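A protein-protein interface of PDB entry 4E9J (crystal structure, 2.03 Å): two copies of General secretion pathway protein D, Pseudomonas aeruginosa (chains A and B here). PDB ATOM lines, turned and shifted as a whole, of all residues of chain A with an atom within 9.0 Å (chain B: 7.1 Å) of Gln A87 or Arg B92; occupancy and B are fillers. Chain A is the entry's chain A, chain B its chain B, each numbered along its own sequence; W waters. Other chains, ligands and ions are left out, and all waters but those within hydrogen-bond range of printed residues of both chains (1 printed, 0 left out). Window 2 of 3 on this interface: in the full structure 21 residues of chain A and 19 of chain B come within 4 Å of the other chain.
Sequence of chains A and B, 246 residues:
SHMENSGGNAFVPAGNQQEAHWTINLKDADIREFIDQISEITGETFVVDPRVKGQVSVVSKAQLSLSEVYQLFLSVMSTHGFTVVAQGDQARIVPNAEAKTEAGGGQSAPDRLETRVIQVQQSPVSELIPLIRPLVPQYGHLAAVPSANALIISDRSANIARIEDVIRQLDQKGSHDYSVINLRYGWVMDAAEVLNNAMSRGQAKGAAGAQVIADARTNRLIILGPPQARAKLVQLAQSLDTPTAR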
ATOM      1  N   PHE A  46     -34.835 -12.275 -10.664  1.00  0.00           N
ATOM      2  CA  PHE A  46     -33.692 -12.539  -9.797  1.00  0.00           C
ATOM      3  C   PHE A  46     -34.056 -13.598  -8.741  1.00  0.00           C
ATOM      4  O   PHE A  46     -35.168 -13.583  -8.235  1.00  0.00           O
ATOM      5  CB  PHE A  46     -33.289 -11.277  -9.034  1.00  0.00           C
ATOM      6  CG  PHE A  46     -32.987 -10.072  -9.891  1.00  0.00           C
ATOM      7  CD1 PHE A  46     -31.826 -10.010 -10.657  1.00  0.00           C
ATOM      8  CD2 PHE A  46     -33.863  -9.007  -9.941  1.00  0.00           C
ATOM      9  CE1 PHE A  46     -31.559  -8.887 -11.455  1.00  0.00           C
ATOM     10  CE2 PHE A  46     -33.591  -7.892 -10.731  1.00  0.00           C
ATOM     11  CZ  PHE A  46     -32.462  -7.851 -11.508  1.00  0.00           C
ATOM     12  N   VAL A  47     -33.115 -14.451  -8.344  1.00  0.00           N
ATOM     13  CA  VAL A  47     -33.279 -15.336  -7.177  1.00  0.00           C
ATOM     14  C   VAL A  47     -32.476 -14.614  -6.100  1.00  0.00           C
ATOM     15  O   VAL A  47     -31.334 -14.262  -6.349  1.00  0.00           O
ATOM     16  CB  VAL A  47     -32.789 -16.790  -7.381  1.00  0.00           C
ATOM     17  CG1 VAL A  47     -32.847 -17.562  -6.068  1.00  0.00           C
ATOM     18  CG2 VAL A  47     -33.628 -17.490  -8.432  1.00  0.00           C
ATOM     19  N   ASP A  49     -30.491 -14.627  -2.696  1.00  0.00           N
ATOM     20  CA  ASP A  49     -29.873 -15.540  -1.722  1.00  0.00           C
ATOM     21  C   ASP A  49     -30.516 -15.325  -0.336  1.00  0.00           C
ATOM     22  O   ASP A  49     -30.755 -14.169   0.040  1.00  0.00           O
ATOM     23  CB  ASP A  49     -28.353 -15.295  -1.664  1.00  0.00           C
ATOM     24  CG  ASP A  49     -27.589 -16.185  -0.711  1.00  0.00           C
ATOM     25  OD1 ASP A  49     -27.516 -15.849   0.472  1.00  0.00           O
ATOM     26  OD2 ASP A  49     -27.000 -17.168  -1.168  1.00  0.00           O
ATOM     27  N   PRO A  50     -30.775 -16.400   0.453  1.00  0.00           N
ATOM     28  CA  PRO A  50     -31.405 -16.212   1.778  1.00  0.00           C
ATOM     29  C   PRO A  50     -30.768 -15.170   2.700  1.00  0.00           C
ATOM     30  O   PRO A  50     -31.465 -14.573   3.509  1.00  0.00           O
ATOM     31  CB  PRO A  50     -31.367 -17.602   2.409  1.00  0.00           C
ATOM     32  CG  PRO A  50     -31.217 -18.550   1.268  1.00  0.00           C
ATOM     33  CD  PRO A  50     -30.586 -17.828   0.131  1.00  0.00           C
ATOM     34  N   ARG A  51     -29.446 -14.948   2.580  1.00  0.00           N
ATOM     35  CA  ARG A  51     -28.707 -13.993   3.415  1.00  0.00           C
ATOM     36  C   ARG A  51     -28.894 -12.520   3.011  1.00  0.00           C
ATOM     37  O   ARG A  51     -28.456 -11.653   3.774  1.00  0.00           O
ATOM     38  CB  ARG A  51     -27.196 -14.299   3.396  1.00  0.00           C
ATOM     39  CG  ARG A  51     -26.779 -15.620   4.008  1.00  0.00           C
ATOM     40  CD  ARG A  51     -25.347 -15.931   3.634  1.00  0.00           C
ATOM     41  NE  ARG A  51     -25.236 -16.374   2.242  1.00  0.00           N
ATOM     42  CZ  ARG A  51     -24.098 -16.718   1.637  1.00  0.00           C
ATOM     43  NH1 ARG A  51     -22.942 -16.664   2.291  1.00  0.00           N
ATOM     44  NH2 ARG A  51     -24.108 -17.120   0.374  1.00  0.00           N
ATOM     45  N   THR A  83     -24.120  -8.312  -4.901  1.00  0.00           N
ATOM     46  CA  THR A  83     -23.778  -8.358  -6.310  1.00  0.00           C
ATOM     47  C   THR A  83     -24.660  -9.374  -7.041  1.00  0.00           C
ATOM     48  O   THR A  83     -25.166 -10.304  -6.407  1.00  0.00           O
ATOM     49  CB  THR A  83     -22.256  -8.653  -6.459  1.00  0.00           C
ATOM     50  OG1 THR A  83     -21.882  -8.557  -7.825  1.00  0.00           O
ATOM     51  CG2 THR A  83     -21.863  -9.993  -5.920  1.00  0.00           C
ATOM     52  N   VAL A  84     -24.830  -9.206  -8.363  1.00  0.00           N
ATOM     53  CA  VAL A  84     -25.624 -10.096  -9.198  1.00  0.00           C
ATOM     54  C   VAL A  84     -24.685 -11.061  -9.917  1.00  0.00           C
ATOM     55  O   VAL A  84     -23.746 -10.623 -10.582  1.00  0.00           O
ATOM     56  CB  VAL A  84     -26.519  -9.326 -10.204  1.00  0.00           C
ATOM     57  CG1 VAL A  84     -27.496 -10.277 -10.904  1.00  0.00           C
ATOM     58  CG2 VAL A  84     -27.261  -8.185  -9.511  1.00  0.00           C
ATOM     59  N   VAL A  85     -24.947 -12.377  -9.787  1.00  0.00           N
ATOM     60  CA  VAL A  85     -24.133 -13.437 -10.388  1.00  0.00           C
ATOM     61  C   VAL A  85     -25.037 -14.360 -11.179  1.00  0.00           C
ATOM     62  O   VAL A  85     -26.245 -14.321 -10.982  1.00  0.00           O
ATOM     63  CB  VAL A  85     -23.340 -14.235  -9.299  1.00  0.00           C
ATOM     64  CG1 VAL A  85     -22.453 -13.310  -8.465  1.00  0.00           C
ATOM     65  CG2 VAL A  85     -24.269 -15.078  -8.399  1.00  0.00           C
ATOM     66  N   ALA A  86     -24.456 -15.208 -12.046  1.00  0.00           N
ATOM     67  CA  ALA A  86     -25.192 -16.227 -12.797  1.00  0.00           C
ATOM     68  C   ALA A  86     -24.947 -17.576 -12.081  1.00  0.00           C
ATOM     69  O   ALA A  86     -23.808 -18.014 -11.978  1.00  0.00           O
ATOM     70  CB  ALA A  86     -24.705 -16.280 -14.241  1.00  0.00           C
ATOM     71  N   GLN A  87     -25.986 -18.193 -11.521  1.00  0.00           N
ATOM     72  CA  GLN A  87     -25.828 -19.457 -10.779  1.00  0.00           C
ATOM     73  C   GLN A  87     -27.055 -20.355 -11.029  1.00  0.00           C
ATOM     74  O   GLN A  87     -28.173 -19.982 -10.671  1.00  0.00           O
ATOM     75  CB  GLN A  87     -25.656 -19.155  -9.264  1.00  0.00           C
ATOM     76  CG  GLN A  87     -25.095 -20.311  -8.435  1.00  0.00           C
ATOM     77  CD  GLN A  87     -25.236 -20.089  -6.941  1.00  0.00           C
ATOM     78  OE1 GLN A  87     -24.818 -19.058  -6.384  1.00  0.00           O
ATOM     79  NE2 GLN A  87     -25.799 -21.065  -6.236  1.00  0.00           N
ATOM     80  N   GLY A  88     -26.837 -21.497 -11.680  1.00  0.00           N
ATOM     81  CA  GLY A  88     -27.891 -22.465 -11.977  1.00  0.00           C
ATOM     82  C   GLY A  88     -28.959 -21.978 -12.935  1.00  0.00           C
ATOM     83  O   GLY A  88     -30.148 -21.994 -12.596  1.00  0.00           O
ATOM     84  N   ASP A  89     -28.534 -21.542 -14.143  1.00  0.00           N
ATOM     85  CA  ASP A  89     -29.396 -21.036 -15.225  1.00  0.00           C
ATOM     86  C   ASP A  89     -30.271 -19.801 -14.845  1.00  0.00           C
ATOM     87  O   ASP A  89     -31.291 -19.564 -15.502  1.00  0.00           O
ATOM     88  CB  ASP A  89     -30.262 -22.172 -15.804  1.00  0.00           C
ATOM     89  N   GLN A  90     -29.861 -18.996 -13.827  1.00  0.00           N
ATOM     90  CA  GLN A  90     -30.631 -17.806 -13.398  1.00  0.00           C
ATOM     91  C   GLN A  90     -29.773 -16.739 -12.715  1.00  0.00           C
ATOM     92  O   GLN A  90     -28.706 -17.044 -12.186  1.00  0.00           O
ATOM     93  CB  GLN A  90     -31.759 -18.221 -12.439  1.00  0.00           C
ATOM     94  N   ALA A  91     -30.264 -15.492 -12.697  1.00  0.00           N
ATOM     95  CA  ALA A  91     -29.577 -14.370 -12.053  1.00  0.00           C
ATOM     96  C   ALA A  91     -29.797 -14.438 -10.539  1.00  0.00           C
ATOM     97  O   ALA A  91     -30.930 -14.540 -10.074  1.00  0.00           O
ATOM     98  CB  ALA A  91     -30.100 -13.055 -12.590  1.00  0.00           C
ATOM     99  N   ARG A  92     -28.712 -14.376  -9.776  1.00  0.00           N
ATOM    100  CA  ARG A  92     -28.762 -14.456  -8.328  1.00  0.00           C
ATOM    101  C   ARG A  92     -28.075 -13.264  -7.705  1.00  0.00           C
ATOM    102  O   ARG A  92     -26.965 -12.904  -8.090  1.00  0.00           O
ATOM    103  CB  ARG A  92     -28.120 -15.757  -7.847  1.00  0.00           C
ATOM    104  CG  ARG A  92     -28.523 -16.165  -6.437  1.00  0.00           C
ATOM    105  CD  ARG A  92     -27.888 -17.494  -6.039  1.00  0.00           C
ATOM    106  NE  ARG A  92     -28.838 -18.349  -5.312  1.00  0.00           N
ATOM    107  CZ  ARG A  92     -28.778 -18.684  -4.023  1.00  0.00           C
ATOM    108  NH1 ARG A  92     -27.776 -18.260  -3.260  1.00  0.00           N
ATOM    109  NH2 ARG A  92     -29.710 -19.464  -3.491  1.00  0.00           N
ATOM    110  N   ILE A  93     -28.742 -12.671  -6.729  1.00  0.00           N
ATOM    111  CA  ILE A  93     -28.259 -11.544  -5.930  1.00  0.00           C
ATOM    112  C   ILE A  93     -27.660 -12.220  -4.696  1.00  0.00           C
ATOM    113  O   ILE A  93     -28.342 -13.017  -4.034  1.00  0.00           O
ATOM    114  CB  ILE A  93     -29.393 -10.541  -5.609  1.00  0.00           C
ATOM    115  CG1 ILE A  93     -30.008  -9.980  -6.952  1.00  0.00           C
ATOM    116  CG2 ILE A  93     -28.905  -9.398  -4.709  1.00  0.00           C
ATOM    117  CD1 ILE A  93     -31.191  -9.090  -6.750  1.00  0.00           C
ATOM    118  N   VAL A  94     -26.369 -11.935  -4.416  1.00  0.00           N
ATOM    119  CA  VAL A  94     -25.601 -12.593  -3.356  1.00  0.00           C
ATOM    120  C   VAL A  94     -24.759 -11.613  -2.526  1.00  0.00           C
ATOM    121  O   VAL A  94     -24.273 -10.629  -3.075  1.00  0.00           O
ATOM    122  CB  VAL A  94     -24.670 -13.671  -3.963  1.00  0.00           C
ATOM    123  CG1 VAL A  94     -25.442 -14.906  -4.367  1.00  0.00           C
ATOM    124  CG2 VAL A  94     -23.867 -13.131  -5.151  1.00  0.00           C
ATOM    125  N   PRO A  95     -24.463 -11.907  -1.236  1.00  0.00           N
ATOM    126  CA  PRO A  95     -23.553 -11.017  -0.490  1.00  0.00           C
ATOM    127  C   PRO A  95     -22.144 -11.054  -1.078  1.00  0.00           C
ATOM    128  O   PRO A  95     -21.680 -12.106  -1.534  1.00  0.00           O
ATOM    129  CB  PRO A  95     -23.624 -11.530   0.955  1.00  0.00           C
ATOM    130  CG  PRO A  95     -24.677 -12.572   0.973  1.00  0.00           C
ATOM    131  CD  PRO A  95     -24.875 -13.060  -0.415  1.00  0.00           C
ATOM    132  N   THR B  45     -10.895 -24.769  -0.322  1.00  0.00           N
ATOM    133  CA  THR B  45     -11.477 -25.609  -1.372  1.00  0.00           C
ATOM    134  C   THR B  45     -12.615 -24.832  -2.038  1.00  0.00           C
ATOM    135  O   THR B  45     -13.342 -24.103  -1.373  1.00  0.00           O
ATOM    136  CB  THR B  45     -11.835 -26.993  -0.817  1.00  0.00           C
ATOM    137  OG1 THR B  45     -12.261 -26.862   0.545  1.00  0.00           O
ATOM    138  CG2 THR B  45     -10.647 -27.948  -0.883  1.00  0.00           C
ATOM    139  N   PHE B  46     -12.697 -24.911  -3.362  1.00  0.00           N
ATOM    140  CA  PHE B  46     -13.718 -24.202  -4.127  1.00  0.00           C
ATOM    141  C   PHE B  46     -14.573 -25.125  -4.916  1.00  0.00           C
ATOM    142  O   PHE B  46     -14.087 -26.087  -5.495  1.00  0.00           O
ATOM    143  CB  PHE B  46     -13.098 -23.187  -5.095  1.00  0.00           C
ATOM    144  CG  PHE B  46     -12.199 -22.184  -4.418  1.00  0.00           C
ATOM    145  CD1 PHE B  46     -12.731 -21.171  -3.632  1.00  0.00           C
ATOM    146  CD2 PHE B  46     -10.825 -22.260  -4.555  1.00  0.00           C
ATOM    147  CE1 PHE B  46     -11.908 -20.248  -3.010  1.00  0.00           C
ATOM    148  CE2 PHE B  46     -10.005 -21.326  -3.943  1.00  0.00           C
ATOM    149  CZ  PHE B  46     -10.551 -20.347  -3.148  1.00  0.00           C
ATOM    150  N   VAL B  47     -15.832 -24.732  -5.029  1.00  0.00           N
ATOM    151  CA  VAL B  47     -16.811 -25.399  -5.858  1.00  0.00           C
ATOM    152  C   VAL B  47     -17.014 -24.404  -7.008  1.00  0.00           C
ATOM    153  O   VAL B  47     -17.362 -23.242  -6.798  1.00  0.00           O
ATOM    154  CB  VAL B  47     -18.050 -25.875  -5.070  1.00  0.00           C
ATOM    155  CG1 VAL B  47     -17.649 -27.038  -4.149  1.00  0.00           C
ATOM    156  CG2 VAL B  47     -18.688 -24.757  -4.249  1.00  0.00           C
ATOM    157  N   VAL B  48     -16.588 -24.825  -8.191  1.00  0.00           N
ATOM    158  CA  VAL B  48     -16.503 -24.000  -9.391  1.00  0.00           C
ATOM    159  C   VAL B  48     -17.709 -24.265 -10.273  1.00  0.00           C
ATOM    160  O   VAL B  48     -17.989 -25.415 -10.635  1.00  0.00           O
ATOM    161  CB  VAL B  48     -15.179 -24.318 -10.119  1.00  0.00           C
ATOM    162  CG1 VAL B  48     -15.006 -23.480 -11.372  1.00  0.00           C
ATOM    163  CG2 VAL B  48     -13.995 -24.151  -9.168  1.00  0.00           C
ATOM    164  N   ASP B  49     -18.423 -23.198 -10.604  1.00  0.00           N
ATOM    165  CA  ASP B  49     -19.594 -23.289 -11.463  1.00  0.00           C
ATOM    166  C   ASP B  49     -19.207 -23.798 -12.873  1.00  0.00           C
ATOM    167  O   ASP B  49     -18.192 -23.354 -13.424  1.00  0.00           O
ATOM    168  CB  ASP B  49     -20.275 -21.923 -11.547  1.00  0.00           C
ATOM    169  CG  ASP B  49     -21.568 -21.897 -12.337  1.00  0.00           C
ATOM    170  OD1 ASP B  49     -21.507 -21.743 -13.571  1.00  0.00           O
ATOM    171  OD2 ASP B  49     -22.636 -21.946 -11.710  1.00  0.00           O
ATOM    172  N   PRO B  50     -20.017 -24.695 -13.484  1.00  0.00           N
ATOM    173  CA  PRO B  50     -19.648 -25.235 -14.808  1.00  0.00           C
ATOM    174  C   PRO B  50     -19.320 -24.203 -15.888  1.00  0.00           C
ATOM    175  O   PRO B  50     -18.552 -24.523 -16.792  1.00  0.00           O
ATOM    176  CB  PRO B  50     -20.864 -26.085 -15.212  1.00  0.00           C
ATOM    177  CG  PRO B  50     -21.608 -26.353 -13.972  1.00  0.00           C
ATOM    178  CD  PRO B  50     -21.236 -25.345 -12.946  1.00  0.00           C
ATOM    179  N   THR B  83     -16.989 -14.001  -9.561  1.00  0.00           N
ATOM    180  CA  THR B  83     -17.196 -13.586  -8.189  1.00  0.00           C
ATOM    181  C   THR B  83     -17.008 -14.814  -7.327  1.00  0.00           C
ATOM    182  O   THR B  83     -17.307 -15.924  -7.759  1.00  0.00           O
ATOM    183  CB  THR B  83     -18.616 -12.996  -8.036  1.00  0.00           C
ATOM    184  OG1 THR B  83     -18.679 -11.772  -8.751  1.00  0.00           O
ATOM    185  CG2 THR B  83     -19.002 -12.731  -6.597  1.00  0.00           C
ATOM    186  N   VAL B  84     -16.542 -14.599  -6.107  1.00  0.00           N
ATOM    187  CA  VAL B  84     -16.327 -15.631  -5.123  1.00  0.00           C
ATOM    188  C   VAL B  84     -17.330 -15.361  -3.994  1.00  0.00           C
ATOM    189  O   VAL B  84     -17.373 -14.239  -3.474  1.00  0.00           O
ATOM    190  CB  VAL B  84     -14.839 -15.612  -4.656  1.00  0.00           C
ATOM    191  CG1 VAL B  84     -14.569 -16.703  -3.625  1.00  0.00           C
ATOM    192  CG2 VAL B  84     -13.911 -15.773  -5.848  1.00  0.00           C
ATOM    193  N   VAL B  85     -18.173 -16.355  -3.665  1.00  0.00           N
ATOM    194  CA  VAL B  85     -19.243 -16.181  -2.669  1.00  0.00           C
ATOM    195  C   VAL B  85     -19.072 -17.172  -1.529  1.00  0.00           C
ATOM    196  O   VAL B  85     -19.053 -18.377  -1.788  1.00  0.00           O
ATOM    197  CB  VAL B  85     -20.645 -16.358  -3.328  1.00  0.00           C
ATOM    198  CG1 VAL B  85     -21.769 -16.034  -2.329  1.00  0.00           C
ATOM    199  CG2 VAL B  85     -20.781 -15.496  -4.587  1.00  0.00           C
ATOM    200  N   ALA B  86     -19.022 -16.668  -0.279  1.00  0.00           N
ATOM    201  CA  ALA B  86     -18.878 -17.474   0.949  1.00  0.00           C
ATOM    202  C   ALA B  86     -19.940 -18.554   1.038  1.00  0.00           C
ATOM    203  O   ALA B  86     -21.088 -18.281   0.718  1.00  0.00           O
ATOM    204  CB  ALA B  86     -18.970 -16.575   2.183  1.00  0.00           C
ATOM    205  N   GLN B  87     -19.553 -19.791   1.407  1.00  0.00           N
ATOM    206  CA  GLN B  87     -20.486 -20.919   1.488  1.00  0.00           C
ATOM    207  C   GLN B  87     -20.067 -21.900   2.594  1.00  0.00           C
ATOM    208  O   GLN B  87     -19.787 -23.071   2.336  1.00  0.00           O
ATOM    209  CB  GLN B  87     -20.605 -21.608   0.117  1.00  0.00           C
ATOM    210  N   GLN B  90     -16.340 -24.115   2.251  1.00  0.00           N
ATOM    211  CA  GLN B  90     -15.968 -23.857   0.855  1.00  0.00           C
ATOM    212  C   GLN B  90     -16.524 -22.518   0.355  1.00  0.00           C
ATOM    213  O   GLN B  90     -17.401 -21.934   0.994  1.00  0.00           O
ATOM    214  CB  GLN B  90     -16.454 -24.998  -0.061  1.00  0.00           C
ATOM    215  N   ALA B  91     -15.978 -22.018  -0.765  1.00  0.00           N
ATOM    216  CA  ALA B  91     -16.433 -20.795  -1.422  1.00  0.00           C
ATOM    217  C   ALA B  91     -16.782 -21.141  -2.867  1.00  0.00           C
ATOM    218  O   ALA B  91     -16.078 -21.902  -3.527  1.00  0.00           O
ATOM    219  CB  ALA B  91     -15.361 -19.719  -1.369  1.00  0.00           C
ATOM    220  N   ARG B  92     -17.856 -20.551  -3.353  1.00  0.00           N
ATOM    221  CA  ARG B  92     -18.395 -20.785  -4.691  1.00  0.00           C
ATOM    222  C   ARG B  92     -17.780 -19.800  -5.728  1.00  0.00           C
ATOM    223  O   ARG B  92     -17.807 -18.605  -5.449  1.00  0.00           O
ATOM    224  CB  ARG B  92     -19.936 -20.620  -4.555  1.00  0.00           C
ATOM    225  CG  ARG B  92     -20.758 -20.734  -5.811  1.00  0.00           C
ATOM    226  CD  ARG B  92     -20.662 -22.098  -6.455  1.00  0.00           C
ATOM    227  NE  ARG B  92     -21.646 -22.258  -7.516  1.00  0.00           N
ATOM    228  CZ  ARG B  92     -21.757 -23.325  -8.300  1.00  0.00           C
ATOM    229  NH1 ARG B  92     -20.936 -24.362  -8.149  1.00  0.00           N
ATOM    230  NH2 ARG B  92     -22.685 -23.365  -9.246  1.00  0.00           N
ATOM    231  N   ILE B  93     -17.231 -20.274  -6.909  1.00  0.00           N
ATOM    232  CA  ILE B  93     -16.721 -19.352  -7.936  1.00  0.00           C
ATOM    233  C   ILE B  93     -17.795 -19.344  -9.021  1.00  0.00           C
ATOM    234  O   ILE B  93     -18.152 -20.415  -9.533  1.00  0.00           O
ATOM    235  CB  ILE B  93     -15.311 -19.762  -8.452  1.00  0.00           C
ATOM    236  CG1 ILE B  93     -14.310 -19.888  -7.243  1.00  0.00           C
ATOM    237  CG2 ILE B  93     -14.802 -18.776  -9.523  1.00  0.00           C
ATOM    238  CD1 ILE B  93     -12.946 -20.351  -7.617  1.00  0.00           C
ATOM    239  N   VAL B  94     -18.336 -18.156  -9.341  1.00  0.00           N
ATOM    240  CA  VAL B  94     -19.464 -17.997 -10.275  1.00  0.00           C
ATOM    241  C   VAL B  94     -19.293 -16.825 -11.255  1.00  0.00           C
ATOM    242  O   VAL B  94     -18.729 -15.816 -10.865  1.00  0.00           O
ATOM    243  CB  VAL B  94     -20.786 -17.800  -9.491  1.00  0.00           C
ATOM    244  CG1 VAL B  94     -21.280 -19.098  -8.904  1.00  0.00           C
ATOM    245  CG2 VAL B  94     -20.661 -16.733  -8.407  1.00  0.00           C
ATOM    246  N   PRO B  95     -19.870 -16.865 -12.475  1.00  0.00           N
ATOM    247  CA  PRO B  95     -19.800 -15.678 -13.339  1.00  0.00           C
ATOM    248  C   PRO B  95     -20.602 -14.517 -12.777  1.00  0.00           C
ATOM    249  O   PRO B  95     -21.650 -14.729 -12.147  1.00  0.00           O
ATOM    250  CB  PRO B  95     -20.377 -16.162 -14.689  1.00  0.00           C
ATOM    251  CG  PRO B  95     -20.571 -17.618 -14.557  1.00  0.00           C
ATOM    252  CD  PRO B  95     -20.657 -17.936 -13.109  1.00  0.00           C
HETATM  253  O   HOH W   1     -19.309 -13.908   0.299  1.00  0.00           O
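Water W1 lies within hydrogen-bond range of the backbone NH (N) of Ala B86 (2.8 Å) and the backbone carbonyl oxygen (O) of Pro A95 (3.5 Å).
The side-chain carboxylate of Asp A49 is in salt-bridge range of the guanidinium group of Arg A51 (2.9 Å).
NH2 of Arg B92 is in salt-bridge range of OD2 of Asp B49 (2.8 Å).
The backbone NH (N) of Val A85 lies within hydrogen-bond range of the backbone carbonyl oxygen (O) of Arg A92, 2.7 Å away.
The backbone NH of Val B85 is in hydrogen-bond range of the backbone carbonyl oxygen of Arg B92 (2.9 Å).
The backbone NH (N) of Thr B83 lies within hydrogen-bond range of the backbone carbonyl oxygen (O) of Val B94, at 2.8 Å.
The backbone NH (N) of Val A94 is in hydrogen-bond range of the backbone carbonyl oxygen (O) of Thr A83, at 2.8 Å.
NH2 of Arg A51 touches CG1 of Val B85, 3.7 Å away.
Val A85 touches Thr B83 (CG1 to CB, 3.9 Å).
CB of Val A85 touches CG2 of Val B94, at 3.8 Å.
CA of Val A85 touches O of Pro B95, at 3.3 Å.
Ala A86 touches Val B94 (O to CB, 3.9 Å).
CG of Gln A87 touches NH2 of Arg B92, at 3.97 Å.
Val B85 touches Val A94 (CG2 to CG2, 3.9 Å).
Val A85 touches Thr B83, but with the chains exchanged Thr A83 does not touch Val B85 (5.8 Å).
Val A85 touches Pro B95, but with the chains exchanged Pro A95 does not touch Val B85 (4.01 Å).
Ala A86 touches Val B94, but with the chains exchanged Val A94 does not touch Ala B86 (7.4 Å).
Ala A86 touches Pro B95, but with the chains exchanged Pro A95 does not touch Ala B86 (5.4 Å).
Positions printed for both chains: 46, 47, 49, 50, 83, 84, 85, 86, 87, 90, 91, 92, 93, 94 and 95.
Of the 9 pairs that touch across the chains among the printed residues, 2 have their exchanged pair printed and touching as well.
Gln A87 touches just one residue of chain B: Arg B92.
Printed residues of chain A within 4 Å of Arg B92: Gln A87 (3.97 Å).
Val B84 touches none of the printed residues of chain A.
No residue of chain A comes within 4 Å of Ala B91.
Of the printed residues of chain A, Pro B95 touches Val A85 and Ala A86.
Of the printed residues of chain B, Ala A86 touches Val B94 and Pro B95.
Arg A92 touches none of the printed residues of chain B.
Ile B93 touches none of the printed residues of chain A.
The nearest residue of chain A that does not touch Arg B92 is Gly A88 (5.2 Å).
The backbone carbonyl oxygen (O) of Pro B95 sits at hydrogen-bond distance from the backbone NH (N) of Ala A86 (2.8 Å).
The guanidinium group of Arg A51 lies within hydrogen-bond range of the backbone carbonyl oxygen of Ala B86 (2.9 Å).
Hydrophobic or aromatic side chains of chain B that line the printed part of chain A: Val B85, Ala B86, Val B94 and Pro B95.
Among the printed residues, no Asp or Glu carboxylate lies within 4 Å of a Lys or Arg side-chain nitrogen of the other chain.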
